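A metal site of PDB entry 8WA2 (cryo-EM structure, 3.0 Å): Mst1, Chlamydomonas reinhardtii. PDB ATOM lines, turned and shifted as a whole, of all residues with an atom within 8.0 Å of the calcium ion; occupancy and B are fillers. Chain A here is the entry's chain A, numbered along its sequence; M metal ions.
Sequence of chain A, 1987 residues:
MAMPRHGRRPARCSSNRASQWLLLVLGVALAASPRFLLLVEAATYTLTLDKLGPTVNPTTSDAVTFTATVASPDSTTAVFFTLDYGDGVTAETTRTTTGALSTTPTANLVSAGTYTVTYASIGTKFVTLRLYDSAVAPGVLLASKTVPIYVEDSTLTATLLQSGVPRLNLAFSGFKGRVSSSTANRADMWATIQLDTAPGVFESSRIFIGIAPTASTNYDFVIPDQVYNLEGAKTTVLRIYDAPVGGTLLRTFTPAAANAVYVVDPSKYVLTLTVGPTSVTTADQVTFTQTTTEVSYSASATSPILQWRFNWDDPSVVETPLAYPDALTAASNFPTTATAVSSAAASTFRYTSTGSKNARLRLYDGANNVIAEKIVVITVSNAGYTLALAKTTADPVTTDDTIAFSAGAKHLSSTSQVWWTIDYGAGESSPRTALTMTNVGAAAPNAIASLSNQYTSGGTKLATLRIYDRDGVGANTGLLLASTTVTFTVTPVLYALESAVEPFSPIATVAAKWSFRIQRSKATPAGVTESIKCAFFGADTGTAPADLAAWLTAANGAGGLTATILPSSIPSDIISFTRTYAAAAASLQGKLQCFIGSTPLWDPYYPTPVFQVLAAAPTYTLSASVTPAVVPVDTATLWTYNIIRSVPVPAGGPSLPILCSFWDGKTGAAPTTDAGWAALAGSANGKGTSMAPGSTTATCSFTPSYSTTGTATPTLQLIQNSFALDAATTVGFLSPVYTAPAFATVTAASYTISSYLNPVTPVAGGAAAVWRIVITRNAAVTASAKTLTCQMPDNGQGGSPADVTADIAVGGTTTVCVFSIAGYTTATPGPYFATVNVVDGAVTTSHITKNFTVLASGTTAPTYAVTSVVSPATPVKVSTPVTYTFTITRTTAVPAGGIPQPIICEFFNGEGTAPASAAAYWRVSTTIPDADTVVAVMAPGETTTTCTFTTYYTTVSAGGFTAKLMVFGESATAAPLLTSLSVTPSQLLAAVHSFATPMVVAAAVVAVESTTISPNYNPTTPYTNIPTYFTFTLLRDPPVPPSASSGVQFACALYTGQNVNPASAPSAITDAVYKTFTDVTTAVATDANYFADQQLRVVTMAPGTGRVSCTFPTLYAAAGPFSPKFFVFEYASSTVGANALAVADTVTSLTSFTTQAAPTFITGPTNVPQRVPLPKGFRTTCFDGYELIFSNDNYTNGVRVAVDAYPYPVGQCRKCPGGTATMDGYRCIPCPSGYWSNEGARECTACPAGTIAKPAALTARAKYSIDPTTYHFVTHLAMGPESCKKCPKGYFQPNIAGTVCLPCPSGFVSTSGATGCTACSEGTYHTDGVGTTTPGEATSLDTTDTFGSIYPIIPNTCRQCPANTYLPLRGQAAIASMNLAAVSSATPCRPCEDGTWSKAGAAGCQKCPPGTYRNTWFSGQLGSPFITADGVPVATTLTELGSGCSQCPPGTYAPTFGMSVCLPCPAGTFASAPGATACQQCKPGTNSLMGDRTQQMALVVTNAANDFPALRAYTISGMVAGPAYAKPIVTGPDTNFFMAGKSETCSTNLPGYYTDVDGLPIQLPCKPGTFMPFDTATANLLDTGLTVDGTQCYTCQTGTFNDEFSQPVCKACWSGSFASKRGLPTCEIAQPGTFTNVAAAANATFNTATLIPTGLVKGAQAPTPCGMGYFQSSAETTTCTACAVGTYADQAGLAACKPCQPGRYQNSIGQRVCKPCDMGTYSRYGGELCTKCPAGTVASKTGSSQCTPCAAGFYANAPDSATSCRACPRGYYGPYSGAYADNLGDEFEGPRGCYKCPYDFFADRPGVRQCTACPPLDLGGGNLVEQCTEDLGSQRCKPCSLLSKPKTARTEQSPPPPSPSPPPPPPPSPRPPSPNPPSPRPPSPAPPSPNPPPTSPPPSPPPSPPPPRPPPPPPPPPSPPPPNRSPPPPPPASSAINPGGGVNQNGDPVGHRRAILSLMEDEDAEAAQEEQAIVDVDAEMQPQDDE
The backbone NH of Thr 933 is in hydrogen-bond range of the side-chain carboxylate of Asp 930.
The backbone NH of Phe 907 lies within hydrogen-bond range of the backbone carbonyl oxygen of Asp 932, 3.0 Å away.
The guanidinium group of Arg 923 lies within salt-bridge range of the side-chain carboxylate of Asp 932 (3.3 Å).
The side-chain carboxylate of Glu 906 lies within hydrogen-bond range of the side-chain hydroxyl of Thr 933 (2.7 Å).
Merely in contact with the calcium ion: Thr 933.
Of the 17 residues printed, 4 come within 4 Å of the calcium ion.
The nearest printed residue that does not touch the calcium ion is Glu 906 (4.3 Å).
OD1 of Asp 932 is bound to the calcium ion (2.3 Å).
OG of Ser 925 is bound to the calcium ion.
The calcium ion is bound by OD2 of Asp 930 (2.5 Å).
The calcium ion has three donor atoms within binding distance.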
ATOM      1  N   CYS A 905     -28.045  21.243 -33.795  1.00  0.00           N
ATOM      2  CA  CYS A 905     -26.776  20.876 -34.408  1.00  0.00           C
ATOM      3  C   CYS A 905     -25.939  20.138 -33.372  1.00  0.00           C
ATOM      4  O   CYS A 905     -25.584  20.719 -32.331  1.00  0.00           O
ATOM      5  CB  CYS A 905     -26.028  22.110 -34.910  1.00  0.00           C
ATOM      6  SG  CYS A 905     -26.981  23.245 -35.960  1.00  0.00           S
ATOM      7  N   GLU A 906     -25.625  18.872 -33.640  1.00  0.00           N
ATOM      8  CA  GLU A 906     -24.696  18.099 -32.839  1.00  0.00           C
ATOM      9  C   GLU A 906     -23.368  18.046 -33.576  1.00  0.00           C
ATOM     10  O   GLU A 906     -23.302  17.573 -34.716  1.00  0.00           O
ATOM     11  CB  GLU A 906     -25.227  16.694 -32.582  1.00  0.00           C
ATOM     12  CG  GLU A 906     -26.564  16.660 -31.859  1.00  0.00           C
ATOM     13  CD  GLU A 906     -26.416  16.428 -30.367  1.00  0.00           C
ATOM     14  OE1 GLU A 906     -25.274  16.206 -29.905  1.00  0.00           O
ATOM     15  OE2 GLU A 906     -27.430  16.496 -29.654  1.00  0.00           O
ATOM     16  N   PHE A 907     -22.309  18.532 -32.933  1.00  0.00           N
ATOM     17  CA  PHE A 907     -21.033  18.770 -33.576  1.00  0.00           C
ATOM     18  C   PHE A 907     -19.950  17.928 -32.919  1.00  0.00           C
ATOM     19  O   PHE A 907     -19.923  17.770 -31.702  1.00  0.00           O
ATOM     20  CB  PHE A 907     -20.680  20.265 -33.482  1.00  0.00           C
ATOM     21  CG  PHE A 907     -19.213  20.561 -33.563  1.00  0.00           C
ATOM     22  CD1 PHE A 907     -18.535  20.458 -34.758  1.00  0.00           C
ATOM     23  CD2 PHE A 907     -18.520  20.974 -32.439  1.00  0.00           C
ATOM     24  CE1 PHE A 907     -17.188  20.740 -34.835  1.00  0.00           C
ATOM     25  CE2 PHE A 907     -17.181  21.257 -32.505  1.00  0.00           C
ATOM     26  CZ  PHE A 907     -16.508  21.141 -33.702  1.00  0.00           C
ATOM     27  N   TYR A 921     -25.093  10.364 -33.471  1.00  0.00           N
ATOM     28  CA  TYR A 921     -24.674  11.708 -33.106  1.00  0.00           C
ATOM     29  C   TYR A 921     -25.591  12.347 -32.078  1.00  0.00           C
ATOM     30  O   TYR A 921     -25.267  13.415 -31.549  1.00  0.00           O
ATOM     31  CB  TYR A 921     -24.589  12.598 -34.345  1.00  0.00           C
ATOM     32  CG  TYR A 921     -23.219  12.655 -34.970  1.00  0.00           C
ATOM     33  CD1 TYR A 921     -22.701  11.572 -35.662  1.00  0.00           C
ATOM     34  CD2 TYR A 921     -22.433  13.794 -34.870  1.00  0.00           C
ATOM     35  CE1 TYR A 921     -21.448  11.621 -36.229  1.00  0.00           C
ATOM     36  CE2 TYR A 921     -21.180  13.853 -35.448  1.00  0.00           C
ATOM     37  CZ  TYR A 921     -20.698  12.758 -36.120  1.00  0.00           C
ATOM     38  OH  TYR A 921     -19.439  12.820 -36.685  1.00  0.00           O
ATOM     39  N   TRP A 922     -26.729  11.725 -31.781  1.00  0.00           N
ATOM     40  CA  TRP A 922     -27.659  12.191 -30.752  1.00  0.00           C
ATOM     41  C   TRP A 922     -27.151  11.724 -29.380  1.00  0.00           C
ATOM     42  O   TRP A 922     -27.653  10.789 -28.774  1.00  0.00           O
ATOM     43  CB  TRP A 922     -29.067  11.687 -31.040  1.00  0.00           C
ATOM     44  CG  TRP A 922     -30.102  12.169 -30.077  1.00  0.00           C
ATOM     45  CD1 TRP A 922     -30.540  11.521 -28.957  1.00  0.00           C
ATOM     46  CD2 TRP A 922     -30.839  13.395 -30.145  1.00  0.00           C
ATOM     47  NE1 TRP A 922     -31.503  12.272 -28.330  1.00  0.00           N
ATOM     48  CE2 TRP A 922     -31.709  13.422 -29.040  1.00  0.00           C
ATOM     49  CE3 TRP A 922     -30.851  14.467 -31.039  1.00  0.00           C
ATOM     50  CZ2 TRP A 922     -32.573  14.485 -28.805  1.00  0.00           C
ATOM     51  CZ3 TRP A 922     -31.721  15.517 -30.806  1.00  0.00           C
ATOM     52  CH2 TRP A 922     -32.566  15.518 -29.699  1.00  0.00           C
ATOM     53  N   ARG A 923     -26.107  12.409 -28.918  1.00  0.00           N
ATOM     54  CA  ARG A 923     -25.523  12.102 -27.623  1.00  0.00           C
ATOM     55  C   ARG A 923     -26.410  12.628 -26.500  1.00  0.00           C
ATOM     56  O   ARG A 923     -27.451  13.263 -26.731  1.00  0.00           O
ATOM     57  CB  ARG A 923     -24.111  12.676 -27.523  1.00  0.00           C
ATOM     58  CG  ARG A 923     -23.033  11.796 -28.123  1.00  0.00           C
ATOM     59  CD  ARG A 923     -22.815  12.123 -29.595  1.00  0.00           C
ATOM     60  NE  ARG A 923     -22.784  13.567 -29.834  1.00  0.00           N
ATOM     61  CZ  ARG A 923     -21.711  14.240 -30.226  1.00  0.00           C
ATOM     62  NH1 ARG A 923     -20.558  13.635 -30.442  1.00  0.00           N
ATOM     63  NH2 ARG A 923     -21.808  15.549 -30.410  1.00  0.00           N
ATOM     64  N   VAL A 924     -25.999  12.371 -25.264  1.00  0.00           N
ATOM     65  CA  VAL A 924     -26.736  12.809 -24.079  1.00  0.00           C
ATOM     66  C   VAL A 924     -26.004  13.990 -23.467  1.00  0.00           C
ATOM     67  O   VAL A 924     -24.790  13.930 -23.216  1.00  0.00           O
ATOM     68  CB  VAL A 924     -26.886  11.659 -23.063  1.00  0.00           C
ATOM     69  CG1 VAL A 924     -25.681  10.743 -23.120  1.00  0.00           C
ATOM     70  CG2 VAL A 924     -27.086  12.203 -21.661  1.00  0.00           C
ATOM     71  N   SER A 925     -26.742  15.070 -23.223  1.00  0.00           N
ATOM     72  CA  SER A 925     -26.176  16.300 -22.681  1.00  0.00           C
ATOM     73  C   SER A 925     -27.016  16.766 -21.502  1.00  0.00           C
ATOM     74  O   SER A 925     -28.227  16.558 -21.460  1.00  0.00           O
ATOM     75  CB  SER A 925     -26.108  17.390 -23.739  1.00  0.00           C
ATOM     76  OG  SER A 925     -25.176  17.068 -24.757  1.00  0.00           O
ATOM     77  N   THR A 926     -26.350  17.420 -20.547  1.00  0.00           N
ATOM     78  CA  THR A 926     -27.053  17.931 -19.372  1.00  0.00           C
ATOM     79  C   THR A 926     -27.893  19.154 -19.720  1.00  0.00           C
ATOM     80  O   THR A 926     -29.115  19.145 -19.595  1.00  0.00           O
ATOM     81  CB  THR A 926     -26.048  18.265 -18.264  1.00  0.00           C
ATOM     82  OG1 THR A 926     -25.033  19.126 -18.805  1.00  0.00           O
ATOM     83  CG2 THR A 926     -25.399  16.998 -17.750  1.00  0.00           C
ATOM     84  N   THR A 927     -27.240  20.226 -20.174  1.00  0.00           N
ATOM     85  CA  THR A 927     -27.913  21.431 -20.628  1.00  0.00           C
ATOM     86  C   THR A 927     -27.724  21.558 -22.132  1.00  0.00           C
ATOM     87  O   THR A 927     -26.606  21.403 -22.631  1.00  0.00           O
ATOM     88  CB  THR A 927     -27.381  22.668 -19.912  1.00  0.00           C
ATOM     89  OG1 THR A 927     -27.032  22.332 -18.562  1.00  0.00           O
ATOM     90  CG2 THR A 927     -28.435  23.761 -19.891  1.00  0.00           C
ATOM     91  N   ILE A 928     -28.815  21.841 -22.851  1.00  0.00           N
ATOM     92  CA  ILE A 928     -28.808  21.702 -24.305  1.00  0.00           C
ATOM     93  C   ILE A 928     -27.777  22.610 -24.978  1.00  0.00           C
ATOM     94  O   ILE A 928     -27.040  22.127 -25.855  1.00  0.00           O
ATOM     95  CB  ILE A 928     -30.220  21.896 -24.866  1.00  0.00           C
ATOM     96  CG1 ILE A 928     -31.226  21.098 -24.040  1.00  0.00           C
ATOM     97  CG2 ILE A 928     -30.276  21.415 -26.298  1.00  0.00           C
ATOM     98  CD1 ILE A 928     -30.934  19.625 -23.995  1.00  0.00           C
ATOM     99  N   PRO A 929     -27.663  23.906 -24.640  1.00  0.00           N
ATOM    100  CA  PRO A 929     -26.614  24.716 -25.281  1.00  0.00           C
ATOM    101  C   PRO A 929     -25.236  24.481 -24.670  1.00  0.00           C
ATOM    102  O   PRO A 929     -24.622  25.382 -24.082  1.00  0.00           O
ATOM    103  CB  PRO A 929     -27.125  26.149 -25.066  1.00  0.00           C
ATOM    104  CG  PRO A 929     -28.522  26.030 -24.558  1.00  0.00           C
ATOM    105  CD  PRO A 929     -28.583  24.734 -23.853  1.00  0.00           C
ATOM    106  N   ASP A 930     -24.736  23.253 -24.794  1.00  0.00           N
ATOM    107  CA  ASP A 930     -23.409  22.921 -24.311  1.00  0.00           C
ATOM    108  C   ASP A 930     -22.380  23.295 -25.377  1.00  0.00           C
ATOM    109  O   ASP A 930     -22.669  24.012 -26.338  1.00  0.00           O
ATOM    110  CB  ASP A 930     -23.333  21.452 -23.908  1.00  0.00           C
ATOM    111  CG  ASP A 930     -23.603  20.498 -25.054  1.00  0.00           C
ATOM    112  OD1 ASP A 930     -23.599  20.937 -26.221  1.00  0.00           O
ATOM    113  OD2 ASP A 930     -23.819  19.304 -24.791  1.00  0.00           O
ATOM    114  N   ALA A 931     -21.145  22.803 -25.226  1.00  0.00           N
ATOM    115  CA  ALA A 931     -20.065  23.146 -26.148  1.00  0.00           C
ATOM    116  C   ALA A 931     -20.135  22.389 -27.472  1.00  0.00           C
ATOM    117  O   ALA A 931     -19.431  22.773 -28.410  1.00  0.00           O
ATOM    118  CB  ALA A 931     -18.709  22.888 -25.489  1.00  0.00           C
ATOM    119  N   ASP A 932     -20.954  21.344 -27.587  1.00  0.00           N
ATOM    120  CA  ASP A 932     -21.036  20.584 -28.824  1.00  0.00           C
ATOM    121  C   ASP A 932     -22.472  20.312 -29.271  1.00  0.00           C
ATOM    122  O   ASP A 932     -22.687  19.448 -30.120  1.00  0.00           O
ATOM    123  CB  ASP A 932     -20.276  19.261 -28.695  1.00  0.00           C
ATOM    124  CG  ASP A 932     -20.914  18.301 -27.713  1.00  0.00           C
ATOM    125  OD1 ASP A 932     -21.746  18.735 -26.907  1.00  0.00           O
ATOM    126  OD2 ASP A 932     -20.559  17.103 -27.752  1.00  0.00           O
ATOM    127  N   THR A 933     -23.453  21.031 -28.731  1.00  0.00           N
ATOM    128  CA  THR A 933     -24.826  20.936 -29.188  1.00  0.00           C
ATOM    129  C   THR A 933     -25.450  22.328 -29.143  1.00  0.00           C
ATOM    130  O   THR A 933     -25.412  22.984 -28.100  1.00  0.00           O
ATOM    131  CB  THR A 933     -25.648  19.972 -28.327  1.00  0.00           C
ATOM    132  OG1 THR A 933     -25.298  18.622 -28.647  1.00  0.00           O
ATOM    133  CG2 THR A 933     -27.131  20.172 -28.574  1.00  0.00           C
ATOM    134  N   VAL A 934     -26.006  22.763 -30.259  1.00  0.00           N
ATOM    135  CA  VAL A 934     -26.526  24.114 -30.398  1.00  0.00           C
ATOM    136  C   VAL A 934     -27.974  24.063 -30.886  1.00  0.00           C
ATOM    137  O   VAL A 934     -28.292  23.308 -31.812  1.00  0.00           O
ATOM    138  CB  VAL A 934     -25.656  24.972 -31.343  1.00  0.00           C
ATOM    139  CG1 VAL A 934     -26.389  26.232 -31.750  1.00  0.00           C
ATOM    140  CG2 VAL A 934     -24.360  25.325 -30.675  1.00  0.00           C
HETATM  141 CA    CA M   1     -23.380  17.318 -26.164  1.00  0.00          CA
